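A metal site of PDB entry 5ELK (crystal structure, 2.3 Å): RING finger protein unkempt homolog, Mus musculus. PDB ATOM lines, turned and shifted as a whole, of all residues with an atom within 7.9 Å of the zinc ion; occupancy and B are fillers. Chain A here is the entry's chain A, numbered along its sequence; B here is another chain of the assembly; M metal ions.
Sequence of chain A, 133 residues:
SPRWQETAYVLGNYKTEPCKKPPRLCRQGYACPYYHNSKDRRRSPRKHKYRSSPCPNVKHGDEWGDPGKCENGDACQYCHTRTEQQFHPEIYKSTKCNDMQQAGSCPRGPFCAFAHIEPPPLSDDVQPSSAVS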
ATOM      1  N   LYS A  93      27.698 -21.038  10.933  1.00  0.00           N
ATOM      2  CA  LYS A  93      26.886 -22.044  11.643  1.00  0.00           C
ATOM      3  C   LYS A  93      27.679 -22.878  12.637  1.00  0.00           C
ATOM      4  O   LYS A  93      27.223 -23.957  13.035  1.00  0.00           O
ATOM      5  CB  LYS A  93      26.180 -22.984  10.657  1.00  0.00           C
ATOM      6  CG  LYS A  93      25.312 -22.294   9.638  1.00  0.00           C
ATOM      7  CD  LYS A  93      24.134 -21.611  10.278  1.00  0.00           C
ATOM      8  CE  LYS A  93      23.067 -21.224   9.277  1.00  0.00           C
ATOM      9  NZ  LYS A  93      21.864 -20.679   9.968  1.00  0.00           N
ATOM     10  N   THR A  95      28.493 -21.931  15.661  1.00  0.00           N
ATOM     11  CA  THR A  95      28.099 -21.550  17.011  1.00  0.00           C
ATOM     12  C   THR A  95      26.596 -21.348  17.083  1.00  0.00           C
ATOM     13  O   THR A  95      26.000 -20.718  16.215  1.00  0.00           O
ATOM     14  CB  THR A  95      28.774 -20.228  17.448  1.00  0.00           C
ATOM     15  OG1 THR A  95      30.207 -20.381  17.405  1.00  0.00           O
ATOM     16  CG2 THR A  95      28.354 -19.830  18.855  1.00  0.00           C
ATOM     17  N   LYS A  96      25.997 -21.855  18.152  1.00  0.00           N
ATOM     18  CA  LYS A  96      24.554 -21.775  18.363  1.00  0.00           C
ATOM     19  C   LYS A  96      24.020 -20.350  18.307  1.00  0.00           C
ATOM     20  O   LYS A  96      24.553 -19.452  18.942  1.00  0.00           O
ATOM     21  CB  LYS A  96      24.202 -22.369  19.730  1.00  0.00           C
ATOM     22  CG  LYS A  96      24.585 -23.828  19.906  1.00  0.00           C
ATOM     23  CD  LYS A  96      24.070 -24.371  21.231  1.00  0.00           C
ATOM     24  CE  LYS A  96      24.860 -23.848  22.429  1.00  0.00           C
ATOM     25  NZ  LYS A  96      24.055 -23.795  23.684  1.00  0.00           N
ATOM     26  N   CYS A  97      22.936 -20.162  17.576  1.00  0.00           N
ATOM     27  CA  CYS A  97      22.243 -18.886  17.557  1.00  0.00           C
ATOM     28  C   CYS A  97      21.533 -18.635  18.882  1.00  0.00           C
ATOM     29  O   CYS A  97      20.657 -19.403  19.312  1.00  0.00           O
ATOM     30  CB  CYS A  97      21.246 -18.857  16.399  1.00  0.00           C
ATOM     31  SG  CYS A  97      20.252 -17.357  16.304  1.00  0.00           S
ATOM     32  N   ASN A  98      21.921 -17.556  19.544  1.00  0.00           N
ATOM     33  CA  ASN A  98      21.416 -17.240  20.869  1.00  0.00           C
ATOM     34  C   ASN A  98      19.947 -16.838  20.855  1.00  0.00           C
ATOM     35  O   ASN A  98      19.186 -17.201  21.749  1.00  0.00           O
ATOM     36  CB  ASN A  98      22.259 -16.110  21.457  1.00  0.00           C
ATOM     37  CG  ASN A  98      22.623 -16.351  22.889  1.00  0.00           C
ATOM     38  OD1 ASN A  98      22.242 -15.573  23.763  1.00  0.00           O
ATOM     39  ND2 ASN A  98      23.358 -17.424  23.155  1.00  0.00           N
ATOM     40  N   ASP A  99      19.555 -16.083  19.845  1.00  0.00           N
ATOM     41  CA  ASP A  99      18.175 -15.614  19.714  1.00  0.00           C
ATOM     42  C   ASP A  99      17.230 -16.795  19.580  1.00  0.00           C
ATOM     43  O   ASP A  99      16.124 -16.791  20.123  1.00  0.00           O
ATOM     44  CB  ASP A  99      18.032 -14.712  18.493  1.00  0.00           C
ATOM     45  CG  ASP A  99      18.959 -13.519  18.535  1.00  0.00           C
ATOM     46  OD1 ASP A  99      20.139 -13.663  18.127  1.00  0.00           O
ATOM     47  OD2 ASP A  99      18.515 -12.435  18.974  1.00  0.00           O
ATOM     48  N   MET A 100      17.671 -17.799  18.830  1.00  0.00           N
ATOM     49  CA  MET A 100      16.853 -18.976  18.584  1.00  0.00           C
ATOM     50  C   MET A 100      16.754 -19.795  19.864  1.00  0.00           C
ATOM     51  O   MET A 100      15.709 -20.361  20.171  1.00  0.00           O
ATOM     52  CB  MET A 100      17.441 -19.818  17.448  1.00  0.00           C
ATOM     53  CG  MET A 100      16.730 -21.156  17.198  1.00  0.00           C
ATOM     54  SD  MET A 100      15.037 -21.002  16.598  1.00  0.00           S
ATOM     55  CE  MET A 100      15.293 -20.535  14.886  1.00  0.00           C
ATOM     56  N   GLN A 101      17.849 -19.819  20.629  1.00  0.00           N
ATOM     57  CA  GLN A 101      17.900 -20.660  21.820  1.00  0.00           C
ATOM     58  C   GLN A 101      17.021 -20.084  22.921  1.00  0.00           C
ATOM     59  O   GLN A 101      16.506 -20.822  23.752  1.00  0.00           O
ATOM     60  CB  GLN A 101      19.329 -20.779  22.323  1.00  0.00           C
ATOM     61  CG  GLN A 101      19.638 -22.128  22.946  1.00  0.00           C
ATOM     62  CD  GLN A 101      21.059 -22.209  23.487  1.00  0.00           C
ATOM     63  OE1 GLN A 101      21.796 -23.139  23.171  1.00  0.00           O
ATOM     64  NE2 GLN A 101      21.443 -21.231  24.306  1.00  0.00           N
ATOM     65  N   SER A 105      12.791 -18.524  17.817  1.00  0.00           N
ATOM     66  CA  SER A 105      12.734 -17.879  16.509  1.00  0.00           C
ATOM     67  C   SER A 105      13.888 -16.875  16.350  1.00  0.00           C
ATOM     68  O   SER A 105      14.330 -16.279  17.322  1.00  0.00           O
ATOM     69  CB  SER A 105      11.396 -17.161  16.327  1.00  0.00           C
ATOM     70  OG  SER A 105      11.425 -15.869  16.912  1.00  0.00           O
ATOM     71  N   CYS A 106      14.359 -16.717  15.118  1.00  0.00           N
ATOM     72  CA  CYS A 106      15.476 -15.806  14.822  1.00  0.00           C
ATOM     73  C   CYS A 106      15.040 -14.791  13.761  1.00  0.00           C
ATOM     74  O   CYS A 106      14.464 -15.167  12.758  1.00  0.00           O
ATOM     75  CB  CYS A 106      16.679 -16.595  14.332  1.00  0.00           C
ATOM     76  SG  CYS A 106      18.086 -15.576  13.875  1.00  0.00           S
ATOM     77  N   PRO A 107      15.329 -13.493  13.986  1.00  0.00           N
ATOM     78  CA  PRO A 107      14.891 -12.458  13.035  1.00  0.00           C
ATOM     79  C   PRO A 107      15.659 -12.449  11.710  1.00  0.00           C
ATOM     80  O   PRO A 107      15.159 -11.952  10.707  1.00  0.00           O
ATOM     81  CB  PRO A 107      15.131 -11.153  13.803  1.00  0.00           C
ATOM     82  CG  PRO A 107      16.158 -11.479  14.831  1.00  0.00           C
ATOM     83  CD  PRO A 107      15.923 -12.909  15.199  1.00  0.00           C
ATOM     84  N   ARG A 108      16.858 -13.015  11.726  1.00  0.00           N
ATOM     85  CA  ARG A 108      17.695 -13.023  10.541  1.00  0.00           C
ATOM     86  C   ARG A 108      17.382 -14.227   9.675  1.00  0.00           C
ATOM     87  O   ARG A 108      17.812 -14.295   8.517  1.00  0.00           O
ATOM     88  CB  ARG A 108      19.164 -13.021  10.957  1.00  0.00           C
ATOM     89  CG  ARG A 108      19.481 -11.971  12.001  1.00  0.00           C
ATOM     90  CD  ARG A 108      20.936 -12.008  12.388  1.00  0.00           C
ATOM     91  NE  ARG A 108      21.229 -13.094  13.316  1.00  0.00           N
ATOM     92  CZ  ARG A 108      20.851 -13.108  14.596  1.00  0.00           C
ATOM     93  NH1 ARG A 108      20.166 -12.092  15.097  1.00  0.00           N
ATOM     94  NH2 ARG A 108      21.165 -14.129  15.381  1.00  0.00           N
ATOM     95  N   GLY A 109      16.647 -15.172  10.249  1.00  0.00           N
ATOM     96  CA  GLY A 109      16.099 -16.298   9.508  1.00  0.00           C
ATOM     97  C   GLY A 109      17.132 -17.019   8.658  1.00  0.00           C
ATOM     98  O   GLY A 109      18.144 -17.476   9.177  1.00  0.00           O
ATOM     99  N   PRO A 110      16.896 -17.129   7.350  1.00  0.00           N
ATOM    100  CA  PRO A 110      17.800 -17.889   6.474  1.00  0.00           C
ATOM    101  C   PRO A 110      19.171 -17.240   6.254  1.00  0.00           C
ATOM    102  O   PRO A 110      20.005 -17.836   5.567  1.00  0.00           O
ATOM    103  CB  PRO A 110      17.025 -17.964   5.157  1.00  0.00           C
ATOM    104  CG  PRO A 110      16.184 -16.724   5.152  1.00  0.00           C
ATOM    105  CD  PRO A 110      15.829 -16.455   6.582  1.00  0.00           C
ATOM    106  N   PHE A 111      19.397 -16.072   6.837  1.00  0.00           N
ATOM    107  CA  PHE A 111      20.651 -15.348   6.634  1.00  0.00           C
ATOM    108  C   PHE A 111      21.358 -15.150   7.952  1.00  0.00           C
ATOM    109  O   PHE A 111      22.314 -14.383   8.044  1.00  0.00           O
ATOM    110  CB  PHE A 111      20.390 -14.015   5.946  1.00  0.00           C
ATOM    111  CG  PHE A 111      19.757 -14.154   4.589  1.00  0.00           C
ATOM    112  CD1 PHE A 111      20.187 -15.116   3.704  1.00  0.00           C
ATOM    113  CD2 PHE A 111      18.703 -13.345   4.221  1.00  0.00           C
ATOM    114  CE1 PHE A 111      19.593 -15.256   2.458  1.00  0.00           C
ATOM    115  CE2 PHE A 111      18.108 -13.484   2.974  1.00  0.00           C
ATOM    116  CZ  PHE A 111      18.560 -14.438   2.098  1.00  0.00           C
ATOM    117  N   CYS A 112      20.902 -15.859   8.981  1.00  0.00           N
ATOM    118  CA  CYS A 112      21.629 -15.926  10.231  1.00  0.00           C
ATOM    119  C   CYS A 112      22.910 -16.702   9.958  1.00  0.00           C
ATOM    120  O   CYS A 112      22.882 -17.714   9.252  1.00  0.00           O
ATOM    121  CB  CYS A 112      20.811 -16.648  11.303  1.00  0.00           C
ATOM    122  SG  CYS A 112      21.570 -16.588  12.958  1.00  0.00           S
ATOM    123  N   ALA A 113      24.019 -16.233  10.521  1.00  0.00           N
ATOM    124  CA  ALA A 113      25.325 -16.883  10.329  1.00  0.00           C
ATOM    125  C   ALA A 113      25.591 -17.896  11.441  1.00  0.00           C
ATOM    126  O   ALA A 113      26.654 -18.532  11.464  1.00  0.00           O
ATOM    127  CB  ALA A 113      26.446 -15.849  10.297  1.00  0.00           C
ATOM    128  N   PHE A 114      24.634 -18.030  12.350  1.00  0.00           N
ATOM    129  CA  PHE A 114      24.743 -18.948  13.479  1.00  0.00           C
ATOM    130  C   PHE A 114      23.846 -20.164  13.329  1.00  0.00           C
ATOM    131  O   PHE A 114      22.924 -20.180  12.517  1.00  0.00           O
ATOM    132  CB  PHE A 114      24.421 -18.210  14.771  1.00  0.00           C
ATOM    133  CG  PHE A 114      25.397 -17.119  15.083  1.00  0.00           C
ATOM    134  CD1 PHE A 114      25.229 -15.847  14.544  1.00  0.00           C
ATOM    135  CD2 PHE A 114      26.484 -17.355  15.887  1.00  0.00           C
ATOM    136  CE1 PHE A 114      26.129 -14.854  14.812  1.00  0.00           C
ATOM    137  CE2 PHE A 114      27.400 -16.353  16.143  1.00  0.00           C
ATOM    138  CZ  PHE A 114      27.208 -15.096  15.618  1.00  0.00           C
ATOM    139  N   ALA A 115      24.116 -21.190  14.124  1.00  0.00           N
ATOM    140  CA  ALA A 115      23.413 -22.453  13.996  1.00  0.00           C
ATOM    141  C   ALA A 115      22.042 -22.399  14.662  1.00  0.00           C
ATOM    142  O   ALA A 115      21.885 -21.884  15.763  1.00  0.00           O
ATOM    143  CB  ALA A 115      24.246 -23.582  14.570  1.00  0.00           C
ATOM    144  N   HIS A 116      21.051 -22.916  13.954  1.00  0.00           N
ATOM    145  CA  HIS A 116      19.726 -23.102  14.523  1.00  0.00           C
ATOM    146  C   HIS A 116      19.607 -24.559  14.921  1.00  0.00           C
ATOM    147  O   HIS A 116      20.590 -25.187  15.300  1.00  0.00           O
ATOM    148  CB  HIS A 116      18.671 -22.666  13.515  1.00  0.00           C
ATOM    149  CG  HIS A 116      18.691 -21.195  13.244  1.00  0.00           C
ATOM    150  ND1 HIS A 116      18.093 -20.610  12.157  1.00  0.00           N
ATOM    151  CD2 HIS A 116      19.283 -20.187  13.948  1.00  0.00           C
ATOM    152  CE1 HIS A 116      18.296 -19.305  12.190  1.00  0.00           C
ATOM    153  NE2 HIS A 116      19.007 -19.016  13.269  1.00  0.00           N
ATOM    154  P     A B   4      31.577 -10.877  16.170  1.00  0.00           P
ATOM    155  OP1   A B   4      32.062  -9.577  15.623  1.00  0.00           O
ATOM    156  OP2   A B   4      32.082 -11.375  17.475  1.00  0.00           O
ATOM    157  O5'   A B   4      29.988 -10.803  16.275  1.00  0.00           O
ATOM    158  C5'   A B   4      29.199 -10.376  15.171  1.00  0.00           C
ATOM    159  C4'   A B   4      27.747 -10.138  15.533  1.00  0.00           C
ATOM    160  O4'   A B   4      27.107 -11.381  15.918  1.00  0.00           O
ATOM    161  C3'   A B   4      27.489  -9.171  16.687  1.00  0.00           C
ATOM    162  O3'   A B   4      26.228  -8.562  16.425  1.00  0.00           O
ATOM    163  C2'   A B   4      27.304 -10.105  17.877  1.00  0.00           C
ATOM    164  O2'   A B   4      26.611  -9.543  18.963  1.00  0.00           O
ATOM    165  C1'   A B   4      26.526 -11.242  17.210  1.00  0.00           C
ATOM    166  N9    A B   4      26.600 -12.536  17.880  1.00  0.00           N
ATOM    167  C8    A B   4      27.685 -13.114  18.484  1.00  0.00           C
ATOM    168  N7    A B   4      27.453 -14.315  18.956  1.00  0.00           N
ATOM    169  C5    A B   4      26.115 -14.560  18.644  1.00  0.00           C
ATOM    170  C6    A B   4      25.274 -15.668  18.876  1.00  0.00           C
ATOM    171  N6    A B   4      25.681 -16.771  19.517  1.00  0.00           N
ATOM    172  N1    A B   4      23.999 -15.598  18.435  1.00  0.00           N
ATOM    173  C2    A B   4      23.615 -14.477  17.788  1.00  0.00           C
ATOM    174  N3    A B   4      24.305 -13.370  17.503  1.00  0.00           N
ATOM    175  C4    A B   4      25.576 -13.463  17.964  1.00  0.00           C
ATOM    176  P     G B   5      26.010  -6.985  16.473  1.00  0.00           P
ATOM    177  OP1   G B   5      27.201  -6.298  17.054  1.00  0.00           O
ATOM    178  OP2   G B   5      24.685  -6.765  17.110  1.00  0.00           O
ATOM    179  O5'   G B   5      25.827  -6.592  14.941  1.00  0.00           O
ATOM    180  C5'   G B   5      26.949  -6.242  14.132  1.00  0.00           C
ATOM    181  C4'   G B   5      26.619  -6.310  12.662  1.00  0.00           C
ATOM    182  O4'   G B   5      26.592  -7.706  12.246  1.00  0.00           O
ATOM    183  C3'   G B   5      25.264  -5.720  12.260  1.00  0.00           C
ATOM    184  O3'   G B   5      25.368  -5.092  10.980  1.00  0.00           O
ATOM    185  C2'   G B   5      24.377  -6.952  12.149  1.00  0.00           C
ATOM    186  O2'   G B   5      23.276  -6.803  11.271  1.00  0.00           O
ATOM    187  C1'   G B   5      25.361  -7.999  11.627  1.00  0.00           C
ATOM    188  N9    G B   5      24.991  -9.374  11.974  1.00  0.00           N
ATOM    189  C8    G B   5      24.960  -9.935  13.234  1.00  0.00           C
ATOM    190  N7    G B   5      24.596 -11.192  13.213  1.00  0.00           N
ATOM    191  C5    G B   5      24.369 -11.473  11.876  1.00  0.00           C
ATOM    192  C6    G B   5      23.960 -12.683  11.242  1.00  0.00           C
ATOM    193  O6    G B   5      23.696 -13.759  11.771  1.00  0.00           O
ATOM    194  N1    G B   5      23.846 -12.537   9.865  1.00  0.00           N
ATOM    195  C2    G B   5      24.126 -11.379   9.177  1.00  0.00           C
ATOM    196  N2    G B   5      23.967 -11.446   7.847  1.00  0.00           N
ATOM    197  N3    G B   5      24.514 -10.243   9.751  1.00  0.00           N
ATOM    198  C4    G B   5      24.619 -10.372  11.089  1.00  0.00           C
HETATM  199 ZN    ZN M   1      19.598 -17.235  14.144  1.00  0.00          ZN
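The side-chain sulfur (SG) of Cys 97 lies close to the guanidinium group (NH2) of Arg 108 (3.5 Å). The backbone NH (N) of Met 100 lies close to the side-chain sulfur (SG) of Cys 97 (3.6 Å). The side-chain sulfur of Cys 112 sits close to O6 of G 5 of chain B (3.7 Å). NE of Arg 108 sits at hydrogen-bond distance from O6 of G 5 of chain B, at 3.0 Å. The side-chain carboxylate of Asp 99 lies within salt-bridge range of the guanidinium group of Arg 108. SG of Cys 112 sits close to NH2 of Arg 108, 3.5 Å away. N of Cys 97 is in hydrogen-bond range of O of Ala 115. The backbone carbonyl oxygen (O) of Cys 112 is in hydrogen-bond range of the side-chain amino group (NZ) of Lys 93 (3.2 Å).
A ring nitrogen (NE2) of His 116 is bound to the zinc ion (2.1 Å). The zinc ion is bound by the side-chain sulfur (SG) of Cys 97 (2.3 Å). The zinc ion is bound by the side-chain sulfur (SG) of Cys 106 (2.3 Å). SG of Cys 112 binds the zinc ion, 2.4 Å away. The zinc ion has four donor atoms within binding distance.
Arg 108 touches the zinc ion (NH2 to ZN, 3.7 Å). Five residues have an atom within 4 Å of the zinc ion: Cys 97, Cys 106, Arg 108, Cys 112 and His 116.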
